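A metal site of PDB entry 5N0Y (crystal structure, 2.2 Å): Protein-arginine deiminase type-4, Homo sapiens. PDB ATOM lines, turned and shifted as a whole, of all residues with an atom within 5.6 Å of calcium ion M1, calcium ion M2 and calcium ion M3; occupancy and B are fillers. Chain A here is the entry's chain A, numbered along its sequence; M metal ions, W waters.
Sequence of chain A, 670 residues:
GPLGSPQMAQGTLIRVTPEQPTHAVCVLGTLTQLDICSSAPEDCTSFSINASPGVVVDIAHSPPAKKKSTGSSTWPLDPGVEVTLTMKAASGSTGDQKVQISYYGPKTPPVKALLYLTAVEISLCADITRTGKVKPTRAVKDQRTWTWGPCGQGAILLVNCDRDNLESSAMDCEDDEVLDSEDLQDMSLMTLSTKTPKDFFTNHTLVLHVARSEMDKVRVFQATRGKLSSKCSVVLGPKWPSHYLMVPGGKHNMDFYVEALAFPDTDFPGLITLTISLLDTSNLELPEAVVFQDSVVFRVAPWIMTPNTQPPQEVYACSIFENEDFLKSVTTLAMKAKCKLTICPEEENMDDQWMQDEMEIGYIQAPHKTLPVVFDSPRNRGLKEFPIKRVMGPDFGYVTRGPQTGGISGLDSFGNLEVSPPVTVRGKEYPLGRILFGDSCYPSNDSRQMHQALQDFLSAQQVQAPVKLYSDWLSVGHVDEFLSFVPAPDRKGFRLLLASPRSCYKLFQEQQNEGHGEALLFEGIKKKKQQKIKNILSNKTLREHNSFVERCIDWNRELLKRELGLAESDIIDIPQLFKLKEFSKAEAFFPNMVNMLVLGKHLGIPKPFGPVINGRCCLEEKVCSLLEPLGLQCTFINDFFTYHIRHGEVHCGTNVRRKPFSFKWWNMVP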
ATOM      1  N   ASN A 160     -24.053  20.512   7.952  1.00  0.00           N
ATOM      2  CA  ASN A 160     -23.225  20.227   9.131  1.00  0.00           C
ATOM      3  C   ASN A 160     -23.813  19.016   9.844  1.00  0.00           C
ATOM      4  O   ASN A 160     -24.330  19.095  10.941  1.00  0.00           O
ATOM      5  CB  ASN A 160     -23.119  21.485  10.002  1.00  0.00           C
ATOM      6  CG  ASN A 160     -22.032  21.398  11.067  1.00  0.00           C
ATOM      7  OD1 ASN A 160     -21.231  20.481  11.072  1.00  0.00           O
ATOM      8  ND2 ASN A 160     -22.029  22.354  11.985  1.00  0.00           N
ATOM      9  N   ASP A 162     -22.163  15.967  10.416  1.00  0.00           N
ATOM     10  CA  ASP A 162     -21.286  15.147  11.279  1.00  0.00           C
ATOM     11  C   ASP A 162     -21.542  15.438  12.781  1.00  0.00           C
ATOM     12  O   ASP A 162     -22.545  16.108  13.157  1.00  0.00           O
ATOM     13  CB  ASP A 162     -19.792  15.290  10.860  1.00  0.00           C
ATOM     14  CG  ASP A 162     -19.217  16.644  11.216  1.00  0.00           C
ATOM     15  OD1 ASP A 162     -20.015  17.506  11.643  1.00  0.00           O
ATOM     16  OD2 ASP A 162     -17.985  16.859  11.033  1.00  0.00           O
ATOM     17  N   ARG A 163     -20.650  14.908  13.634  1.00  0.00           N
ATOM     18  CA  ARG A 163     -20.727  15.059  15.110  1.00  0.00           C
ATOM     19  C   ARG A 163     -19.301  15.210  15.645  1.00  0.00           C
ATOM     20  O   ARG A 163     -18.696  14.258  16.150  1.00  0.00           O
ATOM     21  CB  ARG A 163     -21.454  13.885  15.723  1.00  0.00           C
ATOM     22  CG  ARG A 163     -21.373  13.718  17.233  1.00  0.00           C
ATOM     23  CD  ARG A 163     -22.229  12.539  17.690  1.00  0.00           C
ATOM     24  NE  ARG A 163     -21.733  11.194  17.281  1.00  0.00           N
ATOM     25  CZ  ARG A 163     -22.510  10.133  16.977  1.00  0.00           C
ATOM     26  NH1 ARG A 163     -23.843  10.187  17.020  1.00  0.00           N
ATOM     27  NH2 ARG A 163     -21.960   8.978  16.599  1.00  0.00           N
ATOM     28  N   ASP A 164     -18.751  16.416  15.441  1.00  0.00           N
ATOM     29  CA  ASP A 164     -17.530  16.866  16.107  1.00  0.00           C
ATOM     30  C   ASP A 164     -17.658  16.911  17.674  1.00  0.00           C
ATOM     31  O   ASP A 164     -16.652  16.777  18.382  1.00  0.00           O
ATOM     32  CB  ASP A 164     -17.114  18.234  15.586  1.00  0.00           C
ATOM     33  CG  ASP A 164     -16.608  18.195  14.176  1.00  0.00           C
ATOM     34  OD1 ASP A 164     -15.729  17.362  13.856  1.00  0.00           O
ATOM     35  OD2 ASP A 164     -17.057  19.040  13.370  1.00  0.00           O
ATOM     36  N   ASP A 172     -24.149  17.914  14.689  1.00  0.00           N
ATOM     37  CA  ASP A 172     -23.837  19.297  15.125  1.00  0.00           C
ATOM     38  C   ASP A 172     -24.919  20.351  14.867  1.00  0.00           C
ATOM     39  O   ASP A 172     -25.114  21.236  15.720  1.00  0.00           O
ATOM     40  CB  ASP A 172     -22.529  19.763  14.498  1.00  0.00           C
ATOM     41  CG  ASP A 172     -21.363  18.935  14.925  1.00  0.00           C
ATOM     42  OD1 ASP A 172     -21.422  18.254  16.004  1.00  0.00           O
ATOM     43  OD2 ASP A 172     -20.362  18.987  14.184  1.00  0.00           O
ATOM     44  N   CYS A 173     -25.623  20.255  13.726  1.00  0.00           N
ATOM     45  CA  CYS A 173     -26.550  21.309  13.271  1.00  0.00           C
ATOM     46  C   CYS A 173     -27.969  21.199  13.859  1.00  0.00           C
ATOM     47  O   CYS A 173     -28.864  22.000  13.502  1.00  0.00           O
ATOM     48  CB  CYS A 173     -26.645  21.281  11.744  1.00  0.00           C
ATOM     49  SG  CYS A 173     -27.423  19.797  11.041  1.00  0.00           S
ATOM     50  N   GLU A 174     -28.208  20.201  14.721  1.00  0.00           N
ATOM     51  CA  GLU A 174     -29.537  20.110  15.367  1.00  0.00           C
ATOM     52  C   GLU A 174     -29.823  21.124  16.536  1.00  0.00           C
ATOM     53  O   GLU A 174     -30.950  21.398  16.819  1.00  0.00           O
ATOM     54  CB  GLU A 174     -29.879  18.656  15.691  1.00  0.00           C
ATOM     55  CG  GLU A 174     -30.376  17.933  14.430  1.00  0.00           C
ATOM     56  CD  GLU A 174     -30.308  16.417  14.460  1.00  0.00           C
ATOM     57  OE1 GLU A 174     -29.685  15.858  15.392  1.00  0.00           O
ATOM     58  OE2 GLU A 174     -30.883  15.766  13.553  1.00  0.00           O
ATOM     59  N   ASP A 175     -28.825  21.743  17.129  1.00  0.00           N
ATOM     60  CA  ASP A 175     -29.048  22.703  18.221  1.00  0.00           C
ATOM     61  C   ASP A 175     -28.797  24.102  17.644  1.00  0.00           C
ATOM     62  O   ASP A 175     -28.494  24.228  16.444  1.00  0.00           O
ATOM     63  CB  ASP A 175     -28.095  22.400  19.405  1.00  0.00           C
ATOM     64  CG  ASP A 175     -26.614  22.613  19.054  1.00  0.00           C
ATOM     65  OD1 ASP A 175     -26.302  23.072  17.918  1.00  0.00           O
ATOM     66  OD2 ASP A 175     -25.741  22.294  19.906  1.00  0.00           O
ATOM     67  N   ASP A 176     -28.887  25.124  18.519  1.00  0.00           N
ATOM     68  CA  ASP A 176     -28.617  26.542  18.182  1.00  0.00           C
ATOM     69  C   ASP A 176     -27.288  27.095  18.718  1.00  0.00           C
ATOM     70  O   ASP A 176     -27.207  28.282  19.032  1.00  0.00           O
ATOM     71  CB  ASP A 176     -29.780  27.423  18.662  1.00  0.00           C
ATOM     72  CG  ASP A 176     -31.106  27.087  17.976  1.00  0.00           C
ATOM     73  OD1 ASP A 176     -31.300  27.404  16.774  1.00  0.00           O
ATOM     74  OD2 ASP A 176     -31.978  26.509  18.654  1.00  0.00           O
ATOM     75  N   GLU A 177     -26.249  26.260  18.794  1.00  0.00           N
ATOM     76  CA  GLU A 177     -24.935  26.672  19.319  1.00  0.00           C
ATOM     77  C   GLU A 177     -23.764  25.981  18.607  1.00  0.00           C
ATOM     78  O   GLU A 177     -23.914  24.860  18.088  1.00  0.00           O
ATOM     79  CB  GLU A 177     -24.784  26.358  20.838  1.00  0.00           C
ATOM     80  CG  GLU A 177     -26.065  26.302  21.660  1.00  0.00           C
ATOM     81  CD  GLU A 177     -25.836  26.058  23.145  1.00  0.00           C
ATOM     82  OE1 GLU A 177     -24.907  26.644  23.742  1.00  0.00           O
ATOM     83  OE2 GLU A 177     -26.624  25.279  23.733  1.00  0.00           O
ATOM     84  N   VAL A 178     -22.603  26.644  18.653  1.00  0.00           N
ATOM     85  CA  VAL A 178     -21.319  26.103  18.243  1.00  0.00           C
ATOM     86  C   VAL A 178     -20.615  25.662  19.508  1.00  0.00           C
ATOM     87  O   VAL A 178     -20.083  26.508  20.237  1.00  0.00           O
ATOM     88  CB  VAL A 178     -20.436  27.173  17.587  1.00  0.00           C
ATOM     89  CG1 VAL A 178     -19.080  26.605  17.154  1.00  0.00           C
ATOM     90  CG2 VAL A 178     -21.169  27.818  16.428  1.00  0.00           C
ATOM     91  N   LEU A 179     -20.584  24.352  19.754  1.00  0.00           N
ATOM     92  CA  LEU A 179     -20.055  23.787  21.001  1.00  0.00           C
ATOM     93  C   LEU A 179     -18.582  23.423  20.984  1.00  0.00           C
ATOM     94  O   LEU A 179     -18.032  23.266  22.037  1.00  0.00           O
ATOM     95  CB  LEU A 179     -20.848  22.539  21.388  1.00  0.00           C
ATOM     96  CG  LEU A 179     -22.293  22.805  21.774  1.00  0.00           C
ATOM     97  CD1 LEU A 179     -22.957  21.464  22.064  1.00  0.00           C
ATOM     98  CD2 LEU A 179     -22.396  23.758  22.961  1.00  0.00           C
ATOM     99  N   GLU A 182     -13.586  23.305  16.518  1.00  0.00           N
ATOM    100  CA  GLU A 182     -13.433  22.447  15.350  1.00  0.00           C
ATOM    101  C   GLU A 182     -14.668  22.514  14.428  1.00  0.00           C
ATOM    102  O   GLU A 182     -14.515  22.552  13.218  1.00  0.00           O
ATOM    103  CB  GLU A 182     -13.236  20.977  15.785  1.00  0.00           C
ATOM    104  CG  GLU A 182     -11.868  20.612  16.384  1.00  0.00           C
ATOM    105  CD  GLU A 182     -11.737  20.862  17.890  1.00  0.00           C
ATOM    106  OE1 GLU A 182     -10.578  20.887  18.342  1.00  0.00           O
ATOM    107  OE2 GLU A 182     -12.749  21.048  18.621  1.00  0.00           O
ATOM    108  N   ASP A 183     -15.862  22.520  15.028  1.00  0.00           N
ATOM    109  CA  ASP A 183     -17.126  22.631  14.319  1.00  0.00           C
ATOM    110  C   ASP A 183     -17.079  23.746  13.275  1.00  0.00           C
ATOM    111  O   ASP A 183     -17.563  23.536  12.147  1.00  0.00           O
ATOM    112  CB  ASP A 183     -18.302  22.843  15.289  1.00  0.00           C
ATOM    113  CG  ASP A 183     -19.676  22.601  14.642  1.00  0.00           C
ATOM    114  OD1 ASP A 183     -19.784  21.735  13.772  1.00  0.00           O
ATOM    115  OD2 ASP A 183     -20.667  23.251  15.070  1.00  0.00           O
ATOM    116  N   ASP A 186     -16.228  23.202   9.526  1.00  0.00           N
ATOM    117  CA  ASP A 186     -17.277  22.714   8.662  1.00  0.00           C
ATOM    118  C   ASP A 186     -18.082  23.846   8.029  1.00  0.00           C
ATOM    119  O   ASP A 186     -18.702  23.640   6.997  1.00  0.00           O
ATOM    120  CB  ASP A 186     -18.209  21.783   9.425  1.00  0.00           C
ATOM    121  CG  ASP A 186     -17.513  20.560   9.947  1.00  0.00           C
ATOM    122  OD1 ASP A 186     -16.526  20.092   9.326  1.00  0.00           O
ATOM    123  OD2 ASP A 186     -17.954  20.049  10.996  1.00  0.00           O
ATOM    124  N   PHE A 221     -24.160  32.186  12.420  1.00  0.00           N
ATOM    125  CA  PHE A 221     -23.585  32.570  13.703  1.00  0.00           C
ATOM    126  C   PHE A 221     -22.737  33.800  13.568  1.00  0.00           C
ATOM    127  O   PHE A 221     -21.933  33.880  12.619  1.00  0.00           O
ATOM    128  CB  PHE A 221     -22.680  31.472  14.229  1.00  0.00           C
ATOM    129  CG  PHE A 221     -23.409  30.239  14.627  1.00  0.00           C
ATOM    130  CD1 PHE A 221     -24.027  30.156  15.900  1.00  0.00           C
ATOM    131  CD2 PHE A 221     -23.463  29.140  13.762  1.00  0.00           C
ATOM    132  CE1 PHE A 221     -24.681  28.982  16.284  1.00  0.00           C
ATOM    133  CE2 PHE A 221     -24.146  28.000  14.138  1.00  0.00           C
ATOM    134  CZ  PHE A 221     -24.752  27.923  15.395  1.00  0.00           C
ATOM    135  N   GLU A 259     -23.928  27.428   8.452  1.00  0.00           N
ATOM    136  CA  GLU A 259     -24.096  25.992   8.254  1.00  0.00           C
ATOM    137  C   GLU A 259     -25.446  25.731   7.591  1.00  0.00           C
ATOM    138  O   GLU A 259     -26.415  26.467   7.824  1.00  0.00           O
ATOM    139  CB  GLU A 259     -24.026  25.218   9.610  1.00  0.00           C
ATOM    140  CG  GLU A 259     -25.056  25.703  10.655  1.00  0.00           C
ATOM    141  CD  GLU A 259     -25.050  24.953  12.013  1.00  0.00           C
ATOM    142  OE1 GLU A 259     -24.116  24.143  12.242  1.00  0.00           O
ATOM    143  OE2 GLU A 259     -25.993  25.178  12.859  1.00  0.00           O
ATOM    144  N   LYS A 369     -13.321  22.300   2.986  1.00  0.00           N
ATOM    145  CA  LYS A 369     -13.616  21.118   3.803  1.00  0.00           C
ATOM    146  C   LYS A 369     -14.340  20.032   2.977  1.00  0.00           C
ATOM    147  O   LYS A 369     -15.287  20.328   2.243  1.00  0.00           O
ATOM    148  CB  LYS A 369     -14.466  21.513   5.009  1.00  0.00           C
ATOM    149  CG  LYS A 369     -14.963  20.398   5.873  1.00  0.00           C
ATOM    150  CD  LYS A 369     -13.832  19.580   6.470  1.00  0.00           C
ATOM    151  CE  LYS A 369     -13.187  20.203   7.685  1.00  0.00           C
ATOM    152  NZ  LYS A 369     -12.438  19.159   8.414  1.00  0.00           N
ATOM    153  N   LEU A 371     -15.697  15.936   3.633  1.00  0.00           N
ATOM    154  CA  LEU A 371     -15.795  14.885   4.600  1.00  0.00           C
ATOM    155  C   LEU A 371     -16.754  13.779   4.151  1.00  0.00           C
ATOM    156  O   LEU A 371     -17.634  14.022   3.380  1.00  0.00           O
ATOM    157  CB  LEU A 371     -16.220  15.476   5.912  1.00  0.00           C
ATOM    158  CG  LEU A 371     -17.598  16.144   5.943  1.00  0.00           C
ATOM    159  CD1 LEU A 371     -18.501  15.311   6.813  1.00  0.00           C
ATOM    160  CD2 LEU A 371     -17.602  17.552   6.508  1.00  0.00           C
ATOM    161  N   PRO A 394     -16.760  12.513  14.494  1.00  0.00           N
ATOM    162  CA  PRO A 394     -15.935  13.644  14.075  1.00  0.00           C
ATOM    163  C   PRO A 394     -15.518  13.500  12.639  1.00  0.00           C
ATOM    164  O   PRO A 394     -14.839  12.540  12.297  1.00  0.00           O
ATOM    165  CB  PRO A 394     -14.703  13.567  15.016  1.00  0.00           C
ATOM    166  CG  PRO A 394     -15.140  12.703  16.144  1.00  0.00           C
ATOM    167  CD  PRO A 394     -16.185  11.761  15.616  1.00  0.00           C
ATOM    168  N   ASP A 395     -15.905  14.446  11.813  1.00  0.00           N
ATOM    169  CA  ASP A 395     -15.534  14.437  10.381  1.00  0.00           C
ATOM    170  C   ASP A 395     -16.125  13.257   9.590  1.00  0.00           C
ATOM    171  O   ASP A 395     -15.609  12.877   8.562  1.00  0.00           O
ATOM    172  CB  ASP A 395     -14.009  14.628  10.207  1.00  0.00           C
ATOM    173  CG  ASP A 395     -13.613  16.090  10.347  1.00  0.00           C
ATOM    174  OD1 ASP A 395     -14.450  16.869  10.817  1.00  0.00           O
ATOM    175  OD2 ASP A 395     -12.496  16.505   9.963  1.00  0.00           O
HETATM  176 CA    CA M   1     -24.423  23.109  16.837  1.00  0.00          CA
HETATM  177 CA    CA M   2     -19.405  19.698  12.537  1.00  0.00          CA
HETATM  178 CA    CA M   3     -16.072  18.393  11.206  1.00  0.00          CA
HETATM  179  O   HOH W   1     -23.392  21.557  18.260  1.00  0.00           O
HETATM  180  O   HOH W   2     -23.256  23.692  14.884  1.00  0.00           O
HETATM  181  O   HOH W   3     -14.631  19.777  12.128  1.00  0.00           O
HETATM  182  O   HOH W   4     -26.224  24.251  15.663  1.00  0.00           O
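OE1 of Glu 259 is in hydrogen-bond range of ND2 of Asn 160 (2.8 Å). The side-chain carboxylate of Asp 395 is in salt-bridge range of the side-chain amino group of Lys 369 (3.1 Å). SG of Cys 173 lies within hydrogen-bond range of O of Asn 160.
Of the 21 residues printed, 3 come within 4 Å of calcium ion M1. Along chain A the residues within 4 Å of calcium ion M1 span positions 172 to 177. The nearest printed residue that does not touch calcium ion M1 is Asp 183 (4.2 Å).
Four residues have an atom within 4 Å of calcium ion M3: Asp 162, Asp 164, Asp 186 and Asp 395.
Calcium ion M1 is bound by OD1 of Asp 175 (2.2 Å), O of Glu 177 (2.2 Å), O of Asp 172 (2.3 Å), water W1 (2.3 Å), water W2 (2.3 Å) and water W4 (2.4 Å).
Calcium ion M2 is bound by the side-chain carboxylate (OD2) of Asp 172, the side-chain carboxylate (OD2) of Asp 186, the side-chain carboxylate (OD1) of Asp 183, the side-chain carboxylate (OD1) of Asp 162, the side-chain amide oxygen (OD1) of Asn 160 and the side-chain carboxylate (OD2) of Asp 164.
Calcium ion M3 is bound by water W3 (2.2 Å). Calcium ion M3 is bound by the side-chain carboxylate (OD1) of Asp 395 (2.3 Å). Calcium ion M3 is bound by OD2 of Asp 162. OD2 of Asp 164 is bound to calcium ion M3, 2.5 Å away. The side-chain carboxylate (OD2) of Asp 186 binds calcium ion M3. OD1 of Asp 186 is bound to calcium ion M3, 2.6 Å away. OD1 of Asp 164 binds calcium ion M3 (2.9 Å). Calcium ion M3 has seven donor atoms within binding distance.
Water W2 lies within hydrogen-bond range of the side-chain carboxylate (OD2) of Asp 183 (2.6 Å), the side-chain carboxylate (OE1) of Glu 259 (2.8 Å) and the side-chain amide nitrogen (ND2) of Asn 160 (3.4 Å). Water W4 bridges O of Asp 175 and OE2 of Glu 259.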
